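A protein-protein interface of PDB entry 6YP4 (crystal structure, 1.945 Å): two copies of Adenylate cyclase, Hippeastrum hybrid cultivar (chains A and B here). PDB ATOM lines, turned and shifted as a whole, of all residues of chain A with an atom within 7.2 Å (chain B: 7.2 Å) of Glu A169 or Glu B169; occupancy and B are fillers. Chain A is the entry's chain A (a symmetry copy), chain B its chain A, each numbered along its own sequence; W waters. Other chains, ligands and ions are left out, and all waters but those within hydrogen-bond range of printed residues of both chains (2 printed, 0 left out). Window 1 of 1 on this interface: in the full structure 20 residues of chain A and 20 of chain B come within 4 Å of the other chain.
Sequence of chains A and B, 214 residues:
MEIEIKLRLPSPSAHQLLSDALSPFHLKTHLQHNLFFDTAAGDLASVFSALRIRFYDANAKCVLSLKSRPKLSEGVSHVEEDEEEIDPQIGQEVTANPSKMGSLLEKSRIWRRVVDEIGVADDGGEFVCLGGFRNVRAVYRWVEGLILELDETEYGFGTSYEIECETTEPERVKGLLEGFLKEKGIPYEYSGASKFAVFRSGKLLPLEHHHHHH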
ATOM      1  N   ILE A   3      -7.162   1.741   4.044  1.00  0.00           N
ATOM      2  CA  ILE A   3      -8.391   1.557   4.809  1.00  0.00           C
ATOM      3  C   ILE A   3      -9.395   0.778   3.970  1.00  0.00           C
ATOM      4  O   ILE A   3      -9.719   1.178   2.845  1.00  0.00           O
ATOM      5  CB  ILE A   3      -8.985   2.906   5.245  1.00  0.00           C
ATOM      6  CG1 ILE A   3      -7.969   3.678   6.090  1.00  0.00           C
ATOM      7  CG2 ILE A   3     -10.274   2.686   6.017  1.00  0.00           C
ATOM      8  CD1 ILE A   3      -8.566   4.787   6.928  1.00  0.00           C
ATOM      9  N   ILE A   5     -13.179  -1.716   4.276  1.00  0.00           N
ATOM     10  CA  ILE A   5     -14.282  -2.373   4.966  1.00  0.00           C
ATOM     11  C   ILE A   5     -14.164  -3.856   4.640  1.00  0.00           C
ATOM     12  O   ILE A   5     -13.835  -4.216   3.506  1.00  0.00           O
ATOM     13  CB  ILE A   5     -15.638  -1.796   4.510  1.00  0.00           C
ATOM     14  CG1 ILE A   5     -15.661  -0.270   4.684  1.00  0.00           C
ATOM     15  CG2 ILE A   5     -16.789  -2.455   5.235  1.00  0.00           C
ATOM     16  CD1 ILE A   5     -15.383   0.173   6.071  1.00  0.00           C
ATOM     17  N   GLU A 144     -21.379   5.663  -6.404  1.00  0.00           N
ATOM     18  CA  GLU A 144     -20.313   6.657  -6.246  1.00  0.00           C
ATOM     19  C   GLU A 144     -18.953   6.137  -6.693  1.00  0.00           C
ATOM     20  O   GLU A 144     -17.913   6.605  -6.213  1.00  0.00           O
ATOM     21  CB  GLU A 144     -20.235   7.186  -4.810  1.00  0.00           C
ATOM     22  CG  GLU A 144     -21.579   7.634  -4.283  1.00  0.00           C
ATOM     23  CD  GLU A 144     -21.511   8.264  -2.902  1.00  0.00           C
ATOM     24  OE1 GLU A 144     -22.489   8.102  -2.138  1.00  0.00           O
ATOM     25  OE2 GLU A 144     -20.504   8.938  -2.609  1.00  0.00           O
ATOM     26  N   LEU A 146     -17.550   3.488  -5.970  1.00  0.00           N
ATOM     27  CA  LEU A 146     -16.940   2.569  -5.017  1.00  0.00           C
ATOM     28  C   LEU A 146     -16.702   1.210  -5.660  1.00  0.00           C
ATOM     29  O   LEU A 146     -17.534   0.715  -6.428  1.00  0.00           O
ATOM     30  CB  LEU A 146     -17.844   2.409  -3.788  1.00  0.00           C
ATOM     31  CG  LEU A 146     -18.093   3.666  -2.943  1.00  0.00           C
ATOM     32  CD1 LEU A 146     -19.279   3.477  -1.986  1.00  0.00           C
ATOM     33  CD2 LEU A 146     -16.818   4.054  -2.187  1.00  0.00           C
ATOM     34  N   GLU A 166     -12.347  -0.610  -0.394  1.00  0.00           N
ATOM     35  CA  GLU A 166     -11.353   0.391  -0.022  1.00  0.00           C
ATOM     36  C   GLU A 166     -11.972   1.777  -0.125  1.00  0.00           C
ATOM     37  O   GLU A 166     -12.609   2.107  -1.130  1.00  0.00           O
ATOM     38  CB  GLU A 166     -10.122   0.284  -0.933  1.00  0.00           C
ATOM     39  CG  GLU A 166      -8.775   0.534  -0.240  1.00  0.00           C
ATOM     40  CD  GLU A 166      -8.400   2.008  -0.164  1.00  0.00           C
ATOM     41  OE1 GLU A 166      -8.985   2.806  -0.932  1.00  0.00           O
ATOM     42  OE2 GLU A 166      -7.519   2.365   0.658  1.00  0.00           O
ATOM     43  N   THR A 167     -11.780   2.593   0.905  1.00  0.00           N
ATOM     44  CA  THR A 167     -12.455   3.880   0.939  1.00  0.00           C
ATOM     45  C   THR A 167     -11.678   4.832   1.834  1.00  0.00           C
ATOM     46  O   THR A 167     -10.894   4.413   2.691  1.00  0.00           O
ATOM     47  CB  THR A 167     -13.892   3.722   1.435  1.00  0.00           C
ATOM     48  OG1 THR A 167     -14.535   5.000   1.505  1.00  0.00           O
ATOM     49  CG2 THR A 167     -13.897   3.063   2.821  1.00  0.00           C
ATOM     50  N   THR A 168     -11.894   6.127   1.607  1.00  0.00           N
ATOM     51  CA  THR A 168     -11.396   7.153   2.506  1.00  0.00           C
ATOM     52  C   THR A 168     -12.440   7.565   3.532  1.00  0.00           C
ATOM     53  O   THR A 168     -12.127   8.356   4.426  1.00  0.00           O
ATOM     54  CB  THR A 168     -10.936   8.394   1.723  1.00  0.00           C
ATOM     55  OG1 THR A 168     -12.071   9.036   1.127  1.00  0.00           O
ATOM     56  CG2 THR A 168      -9.961   8.007   0.648  1.00  0.00           C
ATOM     57  N   GLU A 169     -13.669   7.036   3.426  1.00  0.00           N
ATOM     58  CA  GLU A 169     -14.756   7.343   4.349  1.00  0.00           C
ATOM     59  C   GLU A 169     -15.293   6.050   4.979  1.00  0.00           C
ATOM     60  O   GLU A 169     -16.427   5.652   4.712  1.00  0.00           O
ATOM     61  CB  GLU A 169     -15.900   8.082   3.658  1.00  0.00           C
ATOM     62  CG  GLU A 169     -15.496   9.229   2.741  1.00  0.00           C
ATOM     63  CD  GLU A 169     -16.709   9.950   2.165  1.00  0.00           C
ATOM     64  OE1 GLU A 169     -17.562  10.415   2.952  1.00  0.00           O
ATOM     65  OE2 GLU A 169     -16.833  10.009   0.931  1.00  0.00           O
ATOM     66  N   PRO A 170     -14.506   5.410   5.855  1.00  0.00           N
ATOM     67  CA  PRO A 170     -14.914   4.075   6.342  1.00  0.00           C
ATOM     68  C   PRO A 170     -16.259   4.041   7.047  1.00  0.00           C
ATOM     69  O   PRO A 170     -17.047   3.117   6.804  1.00  0.00           O
ATOM     70  CB  PRO A 170     -13.769   3.685   7.293  1.00  0.00           C
ATOM     71  CG  PRO A 170     -13.057   4.975   7.604  1.00  0.00           C
ATOM     72  CD  PRO A 170     -13.203   5.823   6.393  1.00  0.00           C
ATOM     73  N   GLU A 171     -16.563   5.005   7.910  1.00  0.00           N
ATOM     74  CA  GLU A 171     -17.808   4.901   8.662  1.00  0.00           C
ATOM     75  C   GLU A 171     -19.028   5.064   7.763  1.00  0.00           C
ATOM     76  O   GLU A 171     -20.021   4.350   7.929  1.00  0.00           O
ATOM     77  CB  GLU A 171     -17.830   5.917   9.807  1.00  0.00           C
ATOM     78  CG  GLU A 171     -16.780   5.607  10.850  1.00  0.00           C
ATOM     79  CD  GLU A 171     -17.012   4.261  11.520  1.00  0.00           C
ATOM     80  OE1 GLU A 171     -16.021   3.657  11.985  1.00  0.00           O
ATOM     81  OE2 GLU A 171     -18.179   3.811  11.593  1.00  0.00           O
ATOM     82  N   ARG A 172     -18.984   5.981   6.800  1.00  0.00           N
ATOM     83  CA  ARG A 172     -20.175   6.186   5.986  1.00  0.00           C
ATOM     84  C   ARG A 172     -20.341   5.094   4.929  1.00  0.00           C
ATOM     85  O   ARG A 172     -21.465   4.673   4.637  1.00  0.00           O
ATOM     86  CB  ARG A 172     -20.120   7.570   5.339  1.00  0.00           C
ATOM     87  CG  ARG A 172     -21.242   7.849   4.388  1.00  0.00           C
ATOM     88  CD  ARG A 172     -21.021   9.148   3.653  1.00  0.00           C
ATOM     89  NE  ARG A 172     -21.524   9.032   2.308  1.00  0.00           N
ATOM     90  CZ  ARG A 172     -20.722   9.024   1.257  1.00  0.00           C
ATOM     91  NH1 ARG A 172     -19.418   9.160   1.427  1.00  0.00           N
ATOM     92  NH2 ARG A 172     -21.198   8.889   0.031  1.00  0.00           N
ATOM     93  N   VAL A 173     -19.247   4.619   4.335  1.00  0.00           N
ATOM     94  CA  VAL A 173     -19.380   3.586   3.311  1.00  0.00           C
ATOM     95  C   VAL A 173     -19.811   2.273   3.946  1.00  0.00           C
ATOM     96  O   VAL A 173     -20.625   1.527   3.383  1.00  0.00           O
ATOM     97  CB  VAL A 173     -18.071   3.444   2.511  1.00  0.00           C
ATOM     98  CG1 VAL A 173     -18.129   2.226   1.588  1.00  0.00           C
ATOM     99  CG2 VAL A 173     -17.795   4.736   1.697  1.00  0.00           C
ATOM    100  N   LYS A 174     -19.288   1.975   5.134  1.00  0.00           N
ATOM    101  CA  LYS A 174     -19.693   0.754   5.812  1.00  0.00           C
ATOM    102  C   LYS A 174     -21.188   0.774   6.109  1.00  0.00           C
ATOM    103  O   LYS A 174     -21.860  -0.260   6.003  1.00  0.00           O
ATOM    104  CB  LYS A 174     -18.865   0.562   7.079  1.00  0.00           C
ATOM    105  CG  LYS A 174     -19.391  -0.524   7.994  1.00  0.00           C
ATOM    106  CD  LYS A 174     -18.490  -0.694   9.191  1.00  0.00           C
ATOM    107  CE  LYS A 174     -19.065  -0.016  10.416  1.00  0.00           C
ATOM    108  NZ  LYS A 174     -18.203  -0.281  11.604  1.00  0.00           N
ATOM    109  N   GLY A 175     -21.734   1.947   6.450  1.00  0.00           N
ATOM    110  CA  GLY A 175     -23.180   2.075   6.568  1.00  0.00           C
ATOM    111  C   GLY A 175     -23.900   1.788   5.263  1.00  0.00           C
ATOM    112  O   GLY A 175     -24.878   1.037   5.229  1.00  0.00           O
ATOM    113  N   ILE B   3     -16.699   9.945 -10.195  1.00  0.00           N
ATOM    114  CA  ILE B   3     -16.151  11.254  -9.857  1.00  0.00           C
ATOM    115  C   ILE B   3     -14.630  11.178  -9.856  1.00  0.00           C
ATOM    116  O   ILE B   3     -14.042  10.341  -9.160  1.00  0.00           O
ATOM    117  CB  ILE B   3     -16.666  11.739  -8.492  1.00  0.00           C
ATOM    118  CG1 ILE B   3     -18.195  11.815  -8.506  1.00  0.00           C
ATOM    119  CG2 ILE B   3     -16.061  13.091  -8.155  1.00  0.00           C
ATOM    120  CD1 ILE B   3     -18.788  12.675  -7.412  1.00  0.00           C
ATOM    121  N   ILE B   5     -10.895  13.752 -10.083  1.00  0.00           N
ATOM    122  CA  ILE B   5     -10.148  14.999 -10.194  1.00  0.00           C
ATOM    123  C   ILE B   5      -9.293  14.872 -11.448  1.00  0.00           C
ATOM    124  O   ILE B   5      -8.754  13.796 -11.722  1.00  0.00           O
ATOM    125  CB  ILE B   5      -9.286  15.238  -8.938  1.00  0.00           C
ATOM    126  CG1 ILE B   5     -10.151  15.182  -7.670  1.00  0.00           C
ATOM    127  CG2 ILE B   5      -8.524  16.540  -9.032  1.00  0.00           C
ATOM    128  CD1 ILE B   5     -11.279  16.144  -7.679  1.00  0.00           C
ATOM    129  N   GLU B 144      -3.660   7.971   2.164  1.00  0.00           N
ATOM    130  CA  GLU B 144      -4.988   7.410   2.431  1.00  0.00           C
ATOM    131  C   GLU B 144      -5.423   6.400   1.377  1.00  0.00           C
ATOM    132  O   GLU B 144      -6.625   6.199   1.159  1.00  0.00           O
ATOM    133  CB  GLU B 144      -6.048   8.505   2.589  1.00  0.00           C
ATOM    134  CG  GLU B 144      -5.628   9.584   3.560  1.00  0.00           C
ATOM    135  CD  GLU B 144      -6.705  10.624   3.816  1.00  0.00           C
ATOM    136  OE1 GLU B 144      -6.339  11.799   4.047  1.00  0.00           O
ATOM    137  OE2 GLU B 144      -7.895  10.254   3.821  1.00  0.00           O
ATOM    138  N   LEU B 146      -5.378   6.655  -1.696  1.00  0.00           N
ATOM    139  CA  LEU B 146      -5.805   7.270  -2.946  1.00  0.00           C
ATOM    140  C   LEU B 146      -4.934   6.796  -4.101  1.00  0.00           C
ATOM    141  O   LEU B 146      -3.715   6.650  -3.962  1.00  0.00           O
ATOM    142  CB  LEU B 146      -5.728   8.797  -2.833  1.00  0.00           C
ATOM    143  CG  LEU B 146      -6.641   9.462  -1.793  1.00  0.00           C
ATOM    144  CD1 LEU B 146      -6.217  10.912  -1.514  1.00  0.00           C
ATOM    145  CD2 LEU B 146      -8.102   9.383  -2.247  1.00  0.00           C
ATOM    146  N   GLU B 166      -9.660   9.229  -8.766  1.00  0.00           N
ATOM    147  CA  GLU B 166     -11.051   8.885  -8.494  1.00  0.00           C
ATOM    148  C   GLU B 166     -11.294   8.924  -6.992  1.00  0.00           C
ATOM    149  O   GLU B 166     -10.516   8.361  -6.215  1.00  0.00           O
ATOM    150  CB  GLU B 166     -11.375   7.492  -9.054  1.00  0.00           C
ATOM    151  CG  GLU B 166     -12.783   7.342  -9.649  1.00  0.00           C
ATOM    152  CD  GLU B 166     -13.844   7.003  -8.611  1.00  0.00           C
ATOM    153  OE1 GLU B 166     -13.466   6.548  -7.508  1.00  0.00           O
ATOM    154  OE2 GLU B 166     -15.053   7.188  -8.902  1.00  0.00           O
ATOM    155  N   THR B 167     -12.374   9.577  -6.580  1.00  0.00           N
ATOM    156  CA  THR B 167     -12.597   9.776  -5.158  1.00  0.00           C
ATOM    157  C   THR B 167     -14.081   9.992  -4.906  1.00  0.00           C
ATOM    158  O   THR B 167     -14.838  10.366  -5.807  1.00  0.00           O
ATOM    159  CB  THR B 167     -11.782  10.962  -4.644  1.00  0.00           C
ATOM    160  OG1 THR B 167     -12.041  11.175  -3.252  1.00  0.00           O
ATOM    161  CG2 THR B 167     -12.143  12.226  -5.437  1.00  0.00           C
ATOM    162  N   THR B 168     -14.490   9.730  -3.666  1.00  0.00           N
ATOM    163  CA  THR B 168     -15.823  10.085  -3.210  1.00  0.00           C
ATOM    164  C   THR B 168     -15.843  11.434  -2.509  1.00  0.00           C
ATOM    165  O   THR B 168     -16.924  11.913  -2.156  1.00  0.00           O
ATOM    166  CB  THR B 168     -16.384   9.011  -2.263  1.00  0.00           C
ATOM    167  OG1 THR B 168     -15.635   9.008  -1.041  1.00  0.00           O
ATOM    168  CG2 THR B 168     -16.303   7.653  -2.900  1.00  0.00           C
ATOM    169  N   GLU B 169     -14.671  12.057  -2.309  1.00  0.00           N
ATOM    170  CA  GLU B 169     -14.555  13.357  -1.657  1.00  0.00           C
ATOM    171  C   GLU B 169     -13.837  14.349  -2.582  1.00  0.00           C
ATOM    172  O   GLU B 169     -12.716  14.769  -2.293  1.00  0.00           O
ATOM    173  CB  GLU B 169     -13.802  13.264  -0.331  1.00  0.00           C
ATOM    174  CG  GLU B 169     -14.208  12.120   0.588  1.00  0.00           C
ATOM    175  CD  GLU B 169     -13.457  12.163   1.914  1.00  0.00           C
ATOM    176  OE1 GLU B 169     -13.515  13.203   2.604  1.00  0.00           O
ATOM    177  OE2 GLU B 169     -12.774  11.178   2.240  1.00  0.00           O
ATOM    178  N   PRO B 170     -14.491  14.768  -3.674  1.00  0.00           N
ATOM    179  CA  PRO B 170     -13.765  15.579  -4.676  1.00  0.00           C
ATOM    180  C   PRO B 170     -13.184  16.876  -4.141  1.00  0.00           C
ATOM    181  O   PRO B 170     -12.040  17.211  -4.476  1.00  0.00           O
ATOM    182  CB  PRO B 170     -14.832  15.841  -5.752  1.00  0.00           C
ATOM    183  CG  PRO B 170     -16.150  15.551  -5.082  1.00  0.00           C
ATOM    184  CD  PRO B 170     -15.873  14.487  -4.083  1.00  0.00           C
ATOM    185  N   GLU B 171     -13.916  17.625  -3.323  1.00  0.00           N
ATOM    186  CA  GLU B 171     -13.391  18.921  -2.907  1.00  0.00           C
ATOM    187  C   GLU B 171     -12.181  18.774  -1.992  1.00  0.00           C
ATOM    188  O   GLU B 171     -11.213  19.530  -2.116  1.00  0.00           O
ATOM    189  CB  GLU B 171     -14.487  19.754  -2.237  1.00  0.00           C
ATOM    190  CG  GLU B 171     -15.578  20.132  -3.215  1.00  0.00           C
ATOM    191  CD  GLU B 171     -15.061  21.006  -4.347  1.00  0.00           C
ATOM    192  OE1 GLU B 171     -15.664  20.969  -5.441  1.00  0.00           O
ATOM    193  OE2 GLU B 171     -14.064  21.737  -4.143  1.00  0.00           O
ATOM    194  N   ARG B 172     -12.197  17.811  -1.075  1.00  0.00           N
ATOM    195  CA  ARG B 172     -11.072  17.714  -0.154  1.00  0.00           C
ATOM    196  C   ARG B 172      -9.852  17.063  -0.807  1.00  0.00           C
ATOM    197  O   ARG B 172      -8.713  17.460  -0.538  1.00  0.00           O
ATOM    198  CB  ARG B 172     -11.498  16.945   1.097  1.00  0.00           C
ATOM    199  CG  ARG B 172     -10.389  16.687   2.068  1.00  0.00           C
ATOM    200  CD  ARG B 172     -10.841  15.770   3.177  1.00  0.00           C
ATOM    201  NE  ARG B 172      -9.751  14.914   3.569  1.00  0.00           N
ATOM    202  CZ  ARG B 172      -9.761  13.612   3.335  1.00  0.00           C
ATOM    203  NH1 ARG B 172     -10.813  13.059   2.756  1.00  0.00           N
ATOM    204  NH2 ARG B 172      -8.739  12.846   3.676  1.00  0.00           N
ATOM    205  N   VAL B 173     -10.053  16.061  -1.662  1.00  0.00           N
ATOM    206  CA  VAL B 173      -8.904  15.413  -2.287  1.00  0.00           C
ATOM    207  C   VAL B 173      -8.249  16.356  -3.284  1.00  0.00           C
ATOM    208  O   VAL B 173      -7.017  16.410  -3.401  1.00  0.00           O
ATOM    209  CB  VAL B 173      -9.319  14.078  -2.935  1.00  0.00           C
ATOM    210  CG1 VAL B 173      -8.177  13.503  -3.773  1.00  0.00           C
ATOM    211  CG2 VAL B 173      -9.765  13.067  -1.847  1.00  0.00           C
ATOM    212  N   LYS B 174      -9.059  17.129  -4.007  1.00  0.00           N
ATOM    213  CA  LYS B 174      -8.492  18.082  -4.948  1.00  0.00           C
ATOM    214  C   LYS B 174      -7.628  19.107  -4.220  1.00  0.00           C
ATOM    215  O   LYS B 174      -6.576  19.512  -4.731  1.00  0.00           O
ATOM    216  CB  LYS B 174      -9.607  18.747  -5.751  1.00  0.00           C
ATOM    217  CG  LYS B 174      -9.147  19.944  -6.557  1.00  0.00           C
ATOM    218  CD  LYS B 174     -10.286  20.509  -7.366  1.00  0.00           C
ATOM    219  CE  LYS B 174     -10.869  21.746  -6.714  1.00  0.00           C
ATOM    220  NZ  LYS B 174     -11.927  22.336  -7.582  1.00  0.00           N
ATOM    221  N   GLY B 175      -8.036  19.512  -3.013  1.00  0.00           N
ATOM    222  CA  GLY B 175      -7.171  20.344  -2.188  1.00  0.00           C
ATOM    223  C   GLY B 175      -5.864  19.660  -1.838  1.00  0.00           C
ATOM    224  O   GLY B 175      -4.785  20.244  -1.966  1.00  0.00           O
HETATM  225  O   HOH W   1     -12.211   8.840  -2.014  1.00  0.00           O
HETATM  226  O   HOH W   2     -13.837   6.461  -0.591  1.00  0.00           O
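OE2 of Glu A169 is in hydrogen-bond range of OG1 of Thr B168, 2.5 Å away. OG1 of Thr A168 is in hydrogen-bond range of OE2 of Glu B169, 2.5 Å away.
OE1 of Glu A144 lies within salt-bridge range of NH2 of Arg A172 (2.6 Å). NH2 of Arg B172 lies within salt-bridge range of OE1 of Glu B144, at 2.6 Å. The backbone NH of Ile B3 is in hydrogen-bond range of the side-chain carboxylate of Glu B166, at 3.5 Å. N of Ile A3 lies within hydrogen-bond range of OE2 of Glu A166, 3.5 Å away. The side-chain carboxylate (OE1) of Glu A169 is in salt-bridge range of the guanidinium group (NH1) of Arg A172, at 2.7 Å. The side-chain hydroxyl of Thr B167 sits at hydrogen-bond distance from the backbone NH of Glu B169.
Printed residues of chain A that touch a printed residue of chain B: Glu A144, Leu A146, Glu A166, Thr A168 and Glu A169. Hydrophobic or aromatic side chains of chain A within 4 Å of the printed part of chain B: Leu A146. Hydrophobic or aromatic side chains of chain B within 4 Å of the printed part of chain A: Leu B146. Among the printed residues, no Asp or Glu carboxylate lies within 4 Å of a Lys or Arg side-chain nitrogen of the other chain.
Glu A169 touches just these residues of chain B: Thr B168 and Glu B169. Of chain A, only Thr A168 and Glu A169 come within 4 Å of Glu B169. Of the printed residues of chain A, Thr B168 touches Glu A144 (3.8 Å), Leu A146 (3.7 Å) and Glu A169 (2.5 Å). Printed residues of chain A within 4 Å of Leu B146: Thr A168. Of the printed residues of chain B, Leu A146 touches Thr B168 (3.7 Å). Of the printed residues of chain B, Glu A166 touches Glu B144 (3.97 Å). The nearest printed residue of chain B that does not touch Thr A168 is Thr B168 (4.2 Å).
Glu A144 touches Glu B166, and with the chains exchanged Glu A166 touches Glu B144. Glu A144 touches Thr B168, and with the chains exchanged Thr A168 touches Glu B144. Leu A146 touches Thr B168, and with the chains exchanged Thr A168 touches Leu B146. Glu B169 touches its own counterpart, Glu A169. Positions printed for both chains: 3, 5, 144, 146, 166, 167, 168, 169, 170, 171, 172, 173, 174 and 175.
Glu B166 touches Glu A144. O of Glu A144 touches CG2 of Thr B168 (3.8 Å). Leu A146 touches Thr B168 (CD2 to CG2, 3.7 Å). Glu B144 touches Glu A166. Thr A168 touches Glu B144. CD2 of Leu B146 touches CG2 of Thr A168 (3.7 Å). Glu A169 touches Glu B169 (CG to OE2, 3.4 Å).
Water W1 lies within hydrogen-bond range of OG1 of Thr B167 (2.6 Å), N of Thr B168 (3.0 Å) and OG1 of Thr A168 (3.2 Å). Water W2 lies within hydrogen-bond range of OG1 of Thr A167 (2.6 Å), N of Thr A168 (3.0 Å) and OG1 of Thr B168 (3.2 Å).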
